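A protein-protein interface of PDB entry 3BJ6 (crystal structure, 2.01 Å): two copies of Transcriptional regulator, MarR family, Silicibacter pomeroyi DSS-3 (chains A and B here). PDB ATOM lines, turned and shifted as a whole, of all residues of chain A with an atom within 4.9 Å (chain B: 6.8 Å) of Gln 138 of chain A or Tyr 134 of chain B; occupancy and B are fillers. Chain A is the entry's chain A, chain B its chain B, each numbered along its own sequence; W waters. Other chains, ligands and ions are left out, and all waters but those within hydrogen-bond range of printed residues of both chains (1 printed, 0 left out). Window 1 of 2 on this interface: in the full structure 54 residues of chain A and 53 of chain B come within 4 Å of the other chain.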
ATOM      1  N   LEU A  11       8.673  19.802   4.279  1.00  0.00           N
ATOM      2  CA  LEU A  11       9.645  20.881   4.444  1.00  0.00           C
ATOM      3  C   LEU A  11       9.124  22.144   3.762  1.00  0.00           C
ATOM      4  O   LEU A  11       9.242  23.248   4.315  1.00  0.00           O
ATOM      5  CB  LEU A  11      11.022  20.482   3.878  1.00  0.00           C
ATOM      6  CG  LEU A  11      12.135  21.557   4.006  1.00  0.00           C
ATOM      7  CD1 LEU A  11      12.318  21.937   5.485  1.00  0.00           C
ATOM      8  CD2 LEU A  11      13.435  21.050   3.430  1.00  0.00           C
ATOM      9  N   ALA A  14       6.717  23.842   6.005  1.00  0.00           N
ATOM     10  CA  ALA A  14       7.501  24.549   7.017  1.00  0.00           C
ATOM     11  C   ALA A  14       8.102  25.853   6.447  1.00  0.00           C
ATOM     12  O   ALA A  14       8.012  26.923   7.061  1.00  0.00           O
ATOM     13  CB  ALA A  14       8.611  23.635   7.574  1.00  0.00           C
ATOM     14  N   THR A  18       7.288  30.539   7.160  1.00  0.00           N
ATOM     15  CA  THR A  18       8.244  31.608   7.523  1.00  0.00           C
ATOM     16  C   THR A  18       7.605  33.011   7.491  1.00  0.00           C
ATOM     17  O   THR A  18       7.858  33.823   8.385  1.00  0.00           O
ATOM     18  CB  THR A  18       9.516  31.607   6.624  1.00  0.00           C
ATOM     19  OG1 THR A  18      10.031  30.265   6.505  1.00  0.00           O
ATOM     20  CG2 THR A  18      10.613  32.496   7.220  1.00  0.00           C
ATOM     21  N   ALA A 133      17.486  20.503  16.831  1.00  0.00           N
ATOM     22  CA  ALA A 133      17.221  20.189  15.421  1.00  0.00           C
ATOM     23  C   ALA A 133      16.579  21.399  14.735  1.00  0.00           C
ATOM     24  O   ALA A 133      16.995  21.779  13.629  1.00  0.00           O
ATOM     25  CB  ALA A 133      16.311  18.970  15.295  1.00  0.00           C
ATOM     26  N   TYR A 134      15.589  22.022  15.385  1.00  0.00           N
ATOM     27  CA  TYR A 134      15.014  23.214  14.819  1.00  0.00           C
ATOM     28  C   TYR A 134      16.087  24.297  14.533  1.00  0.00           C
ATOM     29  O   TYR A 134      16.142  24.884  13.447  1.00  0.00           O
ATOM     30  CB  TYR A 134      13.921  23.798  15.736  1.00  0.00           C
ATOM     31  CG  TYR A 134      13.356  25.090  15.182  1.00  0.00           C
ATOM     32  CD1 TYR A 134      12.424  25.072  14.138  1.00  0.00           C
ATOM     33  CD2 TYR A 134      13.723  26.350  15.729  1.00  0.00           C
ATOM     34  CE1 TYR A 134      11.910  26.246  13.607  1.00  0.00           C
ATOM     35  CE2 TYR A 134      13.167  27.551  15.193  1.00  0.00           C
ATOM     36  CZ  TYR A 134      12.292  27.485  14.133  1.00  0.00           C
ATOM     37  OH  TYR A 134      11.736  28.638  13.580  1.00  0.00           O
ATOM     38  N   HIS A 135      16.923  24.587  15.523  1.00  0.00           N
ATOM     39  CA  HIS A 135      17.968  25.597  15.355  1.00  0.00           C
ATOM     40  C   HIS A 135      18.926  25.240  14.199  1.00  0.00           C
ATOM     41  O   HIS A 135      19.224  26.084  13.324  1.00  0.00           O
ATOM     42  CB  HIS A 135      18.735  25.762  16.669  1.00  0.00           C
ATOM     43  CG  HIS A 135      19.904  26.695  16.583  1.00  0.00           C
ATOM     44  ND1 HIS A 135      21.180  26.259  16.288  1.00  0.00           N
ATOM     45  CD2 HIS A 135      20.005  28.027  16.814  1.00  0.00           C
ATOM     46  CE1 HIS A 135      22.016  27.287  16.320  1.00  0.00           C
ATOM     47  NE2 HIS A 135      21.331  28.372  16.650  1.00  0.00           N
ATOM     48  N   LYS A 136      19.383  23.990  14.182  1.00  0.00           N
ATOM     49  CA  LYS A 136      20.346  23.519  13.177  1.00  0.00           C
ATOM     50  C   LYS A 136      19.761  23.662  11.768  1.00  0.00           C
ATOM     51  O   LYS A 136      20.424  24.195  10.854  1.00  0.00           O
ATOM     52  CB  LYS A 136      20.750  22.054  13.458  1.00  0.00           C
ATOM     53  CG  LYS A 136      21.909  21.483  12.613  1.00  0.00           C
ATOM     54  CD  LYS A 136      21.943  19.915  12.758  1.00  0.00           C
ATOM     55  CE  LYS A 136      22.873  19.173  11.760  1.00  0.00           C
ATOM     56  NZ  LYS A 136      22.912  17.594  11.905  1.00  0.00           N
ATOM     57  N   VAL A 137      18.528  23.192  11.594  1.00  0.00           N
ATOM     58  CA  VAL A 137      17.871  23.248  10.277  1.00  0.00           C
ATOM     59  C   VAL A 137      17.536  24.700   9.900  1.00  0.00           C
ATOM     60  O   VAL A 137      17.770  25.104   8.763  1.00  0.00           O
ATOM     61  CB  VAL A 137      16.634  22.307  10.217  1.00  0.00           C
ATOM     62  CG1 VAL A 137      15.897  22.430   8.853  1.00  0.00           C
ATOM     63  CG2 VAL A 137      17.073  20.854  10.465  1.00  0.00           C
ATOM     64  N   GLN A 138      17.025  25.489  10.850  1.00  0.00           N
ATOM     65  CA  GLN A 138      16.801  26.915  10.613  1.00  0.00           C
ATOM     66  C   GLN A 138      18.033  27.619  10.051  1.00  0.00           C
ATOM     67  O   GLN A 138      17.940  28.298   9.024  1.00  0.00           O
ATOM     68  CB  GLN A 138      16.347  27.651  11.890  1.00  0.00           C
ATOM     69  CG  GLN A 138      16.042  29.175  11.669  1.00  0.00           C
ATOM     70  CD  GLN A 138      14.614  29.467  11.226  1.00  0.00           C
ATOM     71  OE1 GLN A 138      13.992  28.657  10.535  1.00  0.00           O
ATOM     72  NE2 GLN A 138      14.054  30.623  11.678  1.00  0.00           N
ATOM     73  N   LEU A 139      19.172  27.473  10.724  1.00  0.00           N
ATOM     74  CA  LEU A 139      20.376  28.142  10.269  1.00  0.00           C
ATOM     75  C   LEU A 139      20.906  27.564   8.953  1.00  0.00           C
ATOM     76  O   LEU A 139      21.438  28.312   8.106  1.00  0.00           O
ATOM     77  CB  LEU A 139      21.459  28.146  11.354  1.00  0.00           C
ATOM     78  CG  LEU A 139      21.253  28.896  12.694  1.00  0.00           C
ATOM     79  CD1 LEU A 139      22.619  29.234  13.421  1.00  0.00           C
ATOM     80  CD2 LEU A 139      20.389  30.095  12.604  1.00  0.00           C
ATOM     81  N   ALA A 140      20.810  26.238   8.799  1.00  0.00           N
ATOM     82  CA  ALA A 140      21.218  25.574   7.559  1.00  0.00           C
ATOM     83  C   ALA A 140      20.367  26.013   6.376  1.00  0.00           C
ATOM     84  O   ALA A 140      20.897  26.275   5.312  1.00  0.00           O
ATOM     85  CB  ALA A 140      21.185  24.035   7.715  1.00  0.00           C
ATOM     86  N   LEU A 141      19.049  26.129   6.565  1.00  0.00           N
ATOM     87  CA  LEU A 141      18.187  26.685   5.528  1.00  0.00           C
ATOM     88  C   LEU A 141      18.536  28.108   5.149  1.00  0.00           C
ATOM     89  O   LEU A 141      18.508  28.451   3.970  1.00  0.00           O
ATOM     90  CB  LEU A 141      16.705  26.665   5.937  1.00  0.00           C
ATOM     91  CG  LEU A 141      15.961  25.326   5.807  1.00  0.00           C
ATOM     92  CD1 LEU A 141      14.613  25.498   6.464  1.00  0.00           C
ATOM     93  CD2 LEU A 141      15.822  24.852   4.328  1.00  0.00           C
ATOM     94  N   THR A 142      18.793  28.951   6.151  1.00  0.00           N
ATOM     95  CA  THR A 142      19.186  30.352   5.886  1.00  0.00           C
ATOM     96  C   THR A 142      20.391  30.405   4.932  1.00  0.00           C
ATOM     97  O   THR A 142      20.376  31.126   3.948  1.00  0.00           O
ATOM     98  CB  THR A 142      19.454  31.086   7.189  1.00  0.00           C
ATOM     99  OG1 THR A 142      18.275  30.979   8.008  1.00  0.00           O
ATOM    100  CG2 THR A 142      19.752  32.586   6.924  1.00  0.00           C
ATOM    101  N   GLN B  13      18.239  32.767  18.964  1.00  0.00           N
ATOM    102  CA  GLN B  13      19.079  32.894  17.769  1.00  0.00           C
ATOM    103  C   GLN B  13      18.380  32.336  16.518  1.00  0.00           C
ATOM    104  O   GLN B  13      18.428  32.941  15.448  1.00  0.00           O
ATOM    105  CB  GLN B  13      20.428  32.201  17.984  1.00  0.00           C
ATOM    106  CG  GLN B  13      21.448  32.498  16.911  1.00  0.00           C
ATOM    107  CD  GLN B  13      22.764  31.787  17.188  1.00  0.00           C
ATOM    108  OE1 GLN B  13      22.845  30.556  17.100  1.00  0.00           O
ATOM    109  NE2 GLN B  13      23.799  32.563  17.523  1.00  0.00           N
ATOM    110  N   ALA B  14      17.724  31.186  16.649  1.00  0.00           N
ATOM    111  CA  ALA B  14      16.933  30.620  15.541  1.00  0.00           C
ATOM    112  C   ALA B  14      15.781  31.553  15.146  1.00  0.00           C
ATOM    113  O   ALA B  14      15.548  31.816  13.964  1.00  0.00           O
ATOM    114  CB  ALA B  14      16.387  29.247  15.935  1.00  0.00           C
ATOM    115  N   VAL B  15      15.058  32.052  16.137  1.00  0.00           N
ATOM    116  CA  VAL B  15      13.933  32.951  15.891  1.00  0.00           C
ATOM    117  C   VAL B  15      14.410  34.215  15.174  1.00  0.00           C
ATOM    118  O   VAL B  15      13.749  34.716  14.261  1.00  0.00           O
ATOM    119  CB  VAL B  15      13.166  33.290  17.225  1.00  0.00           C
ATOM    120  CG1 VAL B  15      12.195  34.489  17.031  1.00  0.00           C
ATOM    121  CG2 VAL B  15      12.378  32.054  17.705  1.00  0.00           C
ATOM    122  N   GLN B  16      15.559  34.727  15.598  1.00  0.00           N
ATOM    123  CA  GLN B  16      16.151  35.916  14.964  1.00  0.00           C
ATOM    124  C   GLN B  16      16.509  35.664  13.486  1.00  0.00           C
ATOM    125  O   GLN B  16      16.540  36.615  12.704  1.00  0.00           O
ATOM    126  CB  GLN B  16      17.398  36.319  15.714  1.00  0.00           C
ATOM    127  CG  GLN B  16      17.193  37.115  16.988  1.00  0.00           C
ATOM    128  CD  GLN B  16      18.532  37.552  17.534  1.00  0.00           C
ATOM    129  OE1 GLN B  16      19.430  36.721  17.775  1.00  0.00           O
ATOM    130  NE2 GLN B  16      18.686  38.866  17.734  1.00  0.00           N
ATOM    131  N   ALA B  17      16.786  34.403  13.112  1.00  0.00           N
ATOM    132  CA  ALA B  17      17.149  34.092  11.702  1.00  0.00           C
ATOM    133  C   ALA B  17      15.927  34.132  10.772  1.00  0.00           C
ATOM    134  O   ALA B  17      16.083  34.078   9.572  1.00  0.00           O
ATOM    135  CB  ALA B  17      17.841  32.711  11.588  1.00  0.00           C
ATOM    136  N   THR B  18      14.722  34.206  11.331  1.00  0.00           N
ATOM    137  CA  THR B  18      13.500  34.201  10.519  1.00  0.00           C
ATOM    138  C   THR B  18      13.498  35.339   9.487  1.00  0.00           C
ATOM    139  O   THR B  18      13.128  35.139   8.343  1.00  0.00           O
ATOM    140  CB  THR B  18      12.218  34.316  11.389  1.00  0.00           C
ATOM    141  OG1 THR B  18      12.277  33.377  12.478  1.00  0.00           O
ATOM    142  CG2 THR B  18      10.956  34.001  10.537  1.00  0.00           C
ATOM    143  N   ARG B  19      13.859  36.546   9.914  1.00  0.00           N
ATOM    144  CA  ARG B  19      13.901  37.683   8.992  1.00  0.00           C
ATOM    145  C   ARG B  19      14.916  37.514   7.828  1.00  0.00           C
ATOM    146  O   ARG B  19      14.517  37.621   6.656  1.00  0.00           O
ATOM    147  CB  ARG B  19      14.108  38.992   9.768  1.00  0.00           C
ATOM    148  CG  ARG B  19      14.101  40.263   8.925  1.00  0.00           C
ATOM    149  CD  ARG B  19      14.213  41.467   9.897  1.00  0.00           C
ATOM    150  NE  ARG B  19      14.222  42.777   9.248  1.00  0.00           N
ATOM    151  CZ  ARG B  19      15.308  43.563   9.093  1.00  0.00           C
ATOM    152  NH1 ARG B  19      16.514  43.175   9.526  1.00  0.00           N
ATOM    153  NH2 ARG B  19      15.184  44.754   8.505  1.00  0.00           N
ATOM    154  N   LEU B  21      16.162  34.657   6.834  1.00  0.00           N
ATOM    155  CA  LEU B  21      15.644  33.477   6.124  1.00  0.00           C
ATOM    156  C   LEU B  21      14.589  33.848   5.057  1.00  0.00           C
ATOM    157  O   LEU B  21      14.656  33.395   3.911  1.00  0.00           O
ATOM    158  CB  LEU B  21      15.048  32.464   7.103  1.00  0.00           C
ATOM    159  CG  LEU B  21      14.431  31.179   6.483  1.00  0.00           C
ATOM    160  CD1 LEU B  21      15.382  30.417   5.553  1.00  0.00           C
ATOM    161  CD2 LEU B  21      13.914  30.238   7.575  1.00  0.00           C
ATOM    162  N   ILE B  25      14.911  33.169   1.135  1.00  0.00           N
ATOM    163  CA  ILE B  25      13.927  32.363   0.420  1.00  0.00           C
ATOM    164  C   ILE B  25      13.465  33.146  -0.808  1.00  0.00           C
ATOM    165  O   ILE B  25      13.490  32.633  -1.907  1.00  0.00           O
ATOM    166  CB  ILE B  25      12.714  32.025   1.305  1.00  0.00           C
ATOM    167  CG1 ILE B  25      13.103  31.055   2.427  1.00  0.00           C
ATOM    168  CG2 ILE B  25      11.565  31.406   0.465  1.00  0.00           C
ATOM    169  CD1 ILE B  25      12.060  30.968   3.544  1.00  0.00           C
ATOM    170  N   PHE B 122      18.755  19.792  -0.294  1.00  0.00           N
ATOM    171  CA  PHE B 122      18.980  20.286   1.045  1.00  0.00           C
ATOM    172  C   PHE B 122      18.715  19.165   2.057  1.00  0.00           C
ATOM    173  O   PHE B 122      19.515  18.936   2.972  1.00  0.00           O
ATOM    174  CB  PHE B 122      18.087  21.499   1.355  1.00  0.00           C
ATOM    175  CG  PHE B 122      18.130  21.890   2.818  1.00  0.00           C
ATOM    176  CD1 PHE B 122      19.162  22.703   3.296  1.00  0.00           C
ATOM    177  CD2 PHE B 122      17.195  21.395   3.722  1.00  0.00           C
ATOM    178  CE1 PHE B 122      19.259  23.048   4.652  1.00  0.00           C
ATOM    179  CE2 PHE B 122      17.290  21.715   5.120  1.00  0.00           C
ATOM    180  CZ  PHE B 122      18.325  22.550   5.563  1.00  0.00           C
ATOM    181  N   SER B 128      15.470  12.354   8.481  1.00  0.00           N
ATOM    182  CA  SER B 128      14.077  12.730   8.412  1.00  0.00           C
ATOM    183  C   SER B 128      13.603  13.153   9.811  1.00  0.00           C
ATOM    184  O   SER B 128      12.705  13.979   9.909  1.00  0.00           O
ATOM    185  CB  SER B 128      13.196  11.582   7.871  1.00  0.00           C
ATOM    186  OG  SER B 128      13.397  10.405   8.618  1.00  0.00           O
ATOM    187  N   VAL B 129      14.180  12.573  10.874  1.00  0.00           N
ATOM    188  CA  VAL B 129      13.831  12.961  12.262  1.00  0.00           C
ATOM    189  C   VAL B 129      14.124  14.454  12.523  1.00  0.00           C
ATOM    190  O   VAL B 129      13.278  15.211  13.030  1.00  0.00           O
ATOM    191  CB  VAL B 129      14.563  12.010  13.318  1.00  0.00           C
ATOM    192  CG1 VAL B 129      14.318  12.453  14.734  1.00  0.00           C
ATOM    193  CG2 VAL B 129      14.031  10.596  13.191  1.00  0.00           C
ATOM    194  N   GLU B 130      15.312  14.901  12.145  1.00  0.00           N
ATOM    195  CA  GLU B 130      15.662  16.321  12.250  1.00  0.00           C
ATOM    196  C   GLU B 130      14.711  17.207  11.459  1.00  0.00           C
ATOM    197  O   GLU B 130      14.269  18.258  11.960  1.00  0.00           O
ATOM    198  CB  GLU B 130      17.091  16.547  11.732  1.00  0.00           C
ATOM    199  CG  GLU B 130      18.141  16.052  12.712  1.00  0.00           C
ATOM    200  CD  GLU B 130      19.548  16.125  12.157  1.00  0.00           C
ATOM    201  OE1 GLU B 130      19.753  15.689  10.999  1.00  0.00           O
ATOM    202  OE2 GLU B 130      20.452  16.576  12.898  1.00  0.00           O
ATOM    203  N   LEU B 131      14.433  16.835  10.207  1.00  0.00           N
ATOM    204  CA  LEU B 131      13.506  17.662   9.415  1.00  0.00           C
ATOM    205  C   LEU B 131      12.090  17.683   9.982  1.00  0.00           C
ATOM    206  O   LEU B 131      11.404  18.712   9.915  1.00  0.00           O
ATOM    207  CB  LEU B 131      13.505  17.262   7.940  1.00  0.00           C
ATOM    208  CG  LEU B 131      14.897  17.320   7.319  1.00  0.00           C
ATOM    209  CD1 LEU B 131      14.872  16.630   5.953  1.00  0.00           C
ATOM    210  CD2 LEU B 131      15.379  18.793   7.226  1.00  0.00           C
ATOM    211  N   THR B 132      11.648  16.544  10.520  1.00  0.00           N
ATOM    212  CA  THR B 132      10.335  16.496  11.103  1.00  0.00           C
ATOM    213  C   THR B 132      10.273  17.390  12.350  1.00  0.00           C
ATOM    214  O   THR B 132       9.273  18.066  12.566  1.00  0.00           O
ATOM    215  CB  THR B 132       9.929  15.039  11.427  1.00  0.00           C
ATOM    216  OG1 THR B 132       9.751  14.368  10.179  1.00  0.00           O
ATOM    217  CG2 THR B 132       8.609  15.014  12.166  1.00  0.00           C
ATOM    218  N   ALA B 133      11.336  17.375  13.163  1.00  0.00           N
ATOM    219  CA  ALA B 133      11.442  18.263  14.321  1.00  0.00           C
ATOM    220  C   ALA B 133      11.411  19.736  13.869  1.00  0.00           C
ATOM    221  O   ALA B 133      10.700  20.568  14.474  1.00  0.00           O
ATOM    222  CB  ALA B 133      12.720  17.978  15.081  1.00  0.00           C
ATOM    223  N   TYR B 134      12.149  20.068  12.809  1.00  0.00           N
ATOM    224  CA  TYR B 134      12.066  21.408  12.265  1.00  0.00           C
ATOM    225  C   TYR B 134      10.605  21.800  11.925  1.00  0.00           C
ATOM    226  O   TYR B 134      10.108  22.850  12.338  1.00  0.00           O
ATOM    227  CB  TYR B 134      12.973  21.574  11.027  1.00  0.00           C
ATOM    228  CG  TYR B 134      12.866  22.957  10.443  1.00  0.00           C
ATOM    229  CD1 TYR B 134      13.504  24.049  11.061  1.00  0.00           C
ATOM    230  CD2 TYR B 134      12.123  23.196   9.262  1.00  0.00           C
ATOM    231  CE1 TYR B 134      13.388  25.339  10.539  1.00  0.00           C
ATOM    232  CE2 TYR B 134      12.011  24.516   8.740  1.00  0.00           C
ATOM    233  CZ  TYR B 134      12.624  25.568   9.393  1.00  0.00           C
ATOM    234  OH  TYR B 134      12.558  26.869   8.893  1.00  0.00           O
ATOM    235  N   HIS B 135       9.911  20.955  11.177  1.00  0.00           N
ATOM    236  CA  HIS B 135       8.533  21.264  10.812  1.00  0.00           C
ATOM    237  C   HIS B 135       7.635  21.465  12.051  1.00  0.00           C
ATOM    238  O   HIS B 135       6.852  22.443  12.131  1.00  0.00           O
ATOM    239  CB  HIS B 135       7.995  20.168   9.897  1.00  0.00           C
ATOM    240  CG  HIS B 135       6.533  20.296   9.557  1.00  0.00           C
ATOM    241  ND1 HIS B 135       5.539  19.717  10.320  1.00  0.00           N
ATOM    242  CD2 HIS B 135       5.907  20.874   8.503  1.00  0.00           C
ATOM    243  CE1 HIS B 135       4.360  19.952   9.767  1.00  0.00           C
ATOM    244  NE2 HIS B 135       4.557  20.631   8.645  1.00  0.00           N
ATOM    245  N   LYS B 136       7.729  20.539  13.002  1.00  0.00           N
ATOM    246  CA  LYS B 136       6.881  20.557  14.190  1.00  0.00           C
ATOM    247  C   LYS B 136       7.109  21.848  14.978  1.00  0.00           C
ATOM    248  O   LYS B 136       6.150  22.562  15.342  1.00  0.00           O
ATOM    249  CB  LYS B 136       7.167  19.311  15.059  1.00  0.00           C
ATOM    250  CG  LYS B 136       6.226  19.090  16.287  1.00  0.00           C
ATOM    251  CD  LYS B 136       6.778  17.933  17.169  1.00  0.00           C
ATOM    252  CE  LYS B 136       6.087  17.798  18.530  1.00  0.00           C
ATOM    253  NZ  LYS B 136       6.826  16.871  19.538  1.00  0.00           N
ATOM    254  N   VAL B 137       8.377  22.165  15.215  1.00  0.00           N
ATOM    255  CA  VAL B 137       8.723  23.375  15.966  1.00  0.00           C
ATOM    256  C   VAL B 137       8.348  24.659  15.196  1.00  0.00           C
ATOM    257  O   VAL B 137       7.806  25.587  15.782  1.00  0.00           O
ATOM    258  CB  VAL B 137      10.203  23.339  16.437  1.00  0.00           C
ATOM    259  CG1 VAL B 137      10.569  24.644  17.171  1.00  0.00           C
ATOM    260  CG2 VAL B 137      10.422  22.099  17.381  1.00  0.00           C
ATOM    261  N   GLN B 138       8.645  24.700  13.893  1.00  0.00           N
ATOM    262  CA  GLN B 138       8.263  25.829  13.046  1.00  0.00           C
ATOM    263  C   GLN B 138       6.776  26.158  13.158  1.00  0.00           C
ATOM    264  O   GLN B 138       6.409  27.320  13.376  1.00  0.00           O
ATOM    265  CB  GLN B 138       8.615  25.562  11.560  1.00  0.00           C
ATOM    266  CG  GLN B 138       8.223  26.732  10.600  1.00  0.00           C
ATOM    267  CD  GLN B 138       9.291  27.811  10.479  1.00  0.00           C
ATOM    268  OE1 GLN B 138      10.057  28.056  11.417  1.00  0.00           O
ATOM    269  NE2 GLN B 138       9.394  28.425   9.286  1.00  0.00           N
ATOM    270  N   LEU B 139       5.928  25.145  12.969  1.00  0.00           N
ATOM    271  CA  LEU B 139       4.477  25.338  13.079  1.00  0.00           C
ATOM    272  C   LEU B 139       4.003  25.684  14.490  1.00  0.00           C
ATOM    273  O   LEU B 139       3.094  26.517  14.666  1.00  0.00           O
ATOM    274  CB  LEU B 139       3.703  24.124  12.534  1.00  0.00           C
ATOM    275  CG  LEU B 139       3.848  23.794  11.024  1.00  0.00           C
ATOM    276  CD1 LEU B 139       2.622  23.037  10.461  1.00  0.00           C
ATOM    277  CD2 LEU B 139       4.177  24.959  10.171  1.00  0.00           C
ATOM    278  N   ALA B 140       4.607  25.033  15.489  1.00  0.00           N
ATOM    279  CA  ALA B 140       4.278  25.313  16.899  1.00  0.00           C
ATOM    280  C   ALA B 140       4.653  26.740  17.301  1.00  0.00           C
ATOM    281  O   ALA B 140       3.868  27.430  17.965  1.00  0.00           O
ATOM    282  CB  ALA B 140       4.945  24.274  17.834  1.00  0.00           C
ATOM    283  N   LEU B 141       5.817  27.214  16.861  1.00  0.00           N
ATOM    284  CA  LEU B 141       6.199  28.614  17.072  1.00  0.00           C
ATOM    285  C   LEU B 141       5.250  29.591  16.395  1.00  0.00           C
ATOM    286  O   LEU B 141       4.962  30.628  16.950  1.00  0.00           O
ATOM    287  CB  LEU B 141       7.620  28.921  16.540  1.00  0.00           C
ATOM    288  CG  LEU B 141       8.822  28.484  17.402  1.00  0.00           C
ATOM    289  CD1 LEU B 141      10.062  28.629  16.604  1.00  0.00           C
ATOM    290  CD2 LEU B 141       8.916  29.293  18.706  1.00  0.00           C
HETATM  291  O   HOH W   1      11.509  30.330  10.163  1.00  0.00           O
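O of Ala 14 of chain A lies within hydrogen-bond range of NE2 of Gln 138 of chain B (3.0 Å). OG1 of Thr 18 of chain A is in hydrogen-bond range of NE2 of Gln 138 of chain B, at 3.4 Å. OE1 of Gln 138 of chain B is in hydrogen-bond range of OH of Tyr 134 of chain A (2.8 Å). A ring nitrogen (NE2) of His 135 of chain A sits at hydrogen-bond distance from the side-chain amide oxygen (OE1) of Gln 13 of chain B, at 2.7 Å. The side-chain carboxylate of Glu 130 of chain B lies within salt-bridge range of the side-chain amino group of Lys 136 of chain A, 2.8 Å away. O of Ala 14 of chain B sits at hydrogen-bond distance from NE2 of Gln 138 of chain A, 3.0 Å away. NE2 of Gln 138 of chain A lies within hydrogen-bond range of OG1 of Thr 18 of chain B, 3.4 Å away. The side-chain amide oxygen (OE1) of Gln 138 of chain A lies within hydrogen-bond range of the side-chain hydroxyl (OH) of Tyr 134 of chain B (2.8 Å).
The backbone carbonyl oxygen of Gln 138 of chain A lies within hydrogen-bond range of the side-chain hydroxyl of Thr 142 of chain A (2.9 Å). The backbone carbonyl oxygen (O) of Val 15 of chain B sits at hydrogen-bond distance from the side-chain hydroxyl (OG1) of Thr 18 of chain B (2.7 Å).
CD2 of Leu 11 of chain A touches CD2 of Phe 122 of chain B, 3.8 Å away. O of Glu 130 of chain B touches CB of Ala 133 of chain A, 3.97 Å away. CB of Ala 133 of chain A touches CB of Ala 133 of chain B, 3.7 Å away. CD1 of Tyr 134 of chain A touches CD1 of Tyr 134 of chain B, at 3.4 Å. CG of Tyr 134 of chain A touches CG1 of Val 137 of chain B (3.5 Å). CD2 of His 135 of chain A touches N of Ala 14 of chain B, at 3.9 Å. Tyr 134 of chain B touches Val 137 of chain A (CG to CG1, 3.5 Å). CD2 of Leu 139 of chain A touches CB of Ala 17 of chain B, at 3.8 Å. Leu 21 of chain B touches Leu 141 of chain A (CD1 to C, 3.9 Å). OG1 of Thr 142 of chain A touches CB of Leu 21 of chain B (3.7 Å).
Printed residues of chain B within 4 Å of Ala 14 of chain A: Tyr 134, His 135 and Gln 138. Of the printed residues of chain B, His 135 of chain A touches Gln 13 and Ala 14. Of chain B, only Ala 14 (3.0 Å), Ala 17 (3.97 Å), Thr 18 (3.4 Å), Leu 21 (3.4 Å) and Tyr 134 (2.8 Å) come within 4 Å of Gln 138 of chain A. Printed residues of chain B within 4 Å of Leu 141 of chain A: Leu 21 (3.9 Å), Phe 122 (3.6 Å) and Tyr 134 (3.5 Å). Of the printed residues of chain A, Ile 25 of chain B touches Thr 18. Of the printed residues of chain A, Tyr 134 of chain B touches Leu 11, Ala 14, Tyr 134, Val 137, Gln 138 and Leu 141. Lys 136 of chain B touches none of the printed residues of chain A.
Hydrophobic or aromatic side chains of chain B that line the printed part of chain A: Ala 14, Ala 17, Leu 21, Ile 25, Phe 122, Ala 133, Tyr 134, His 135, Val 137 and Leu 141. Of the 13 printed residues of chain A, 13 touch a printed residue of chain B. Hydrophobic or aromatic side chains of chain A that line the printed part of chain B: Leu 11, Ala 14, Ala 133, Tyr 134, His 135, Val 137, Leu 139, Ala 140 and Leu 141. Among the printed residues, 31 pairs touch across the chains.
Ala 14 of chain A touches His 135 of chain B, and with the chains exchanged His 135 of chain A touches Ala 14 of chain B. Thr 18 of chain A touches its own counterpart, Thr 18 of chain B. Tyr 134 of chain A touches Val 137 of chain B, and with the chains exchanged Val 137 of chain A touches Tyr 134 of chain B. Tyr 134 of chain A touches Leu 141 of chain B, and with the chains exchanged Leu 141 of chain A touches Tyr 134 of chain B. 11 positions are printed for both chains. Of the 31 pairs that touch across the chains among the printed residues, 17 have their exchanged pair printed and touching as well.
Water W1 bridges the side-chain amide oxygen (OE1) of Gln 138 of chain B and the side-chain amide nitrogen (NE2) of Gln 138 of chain A.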
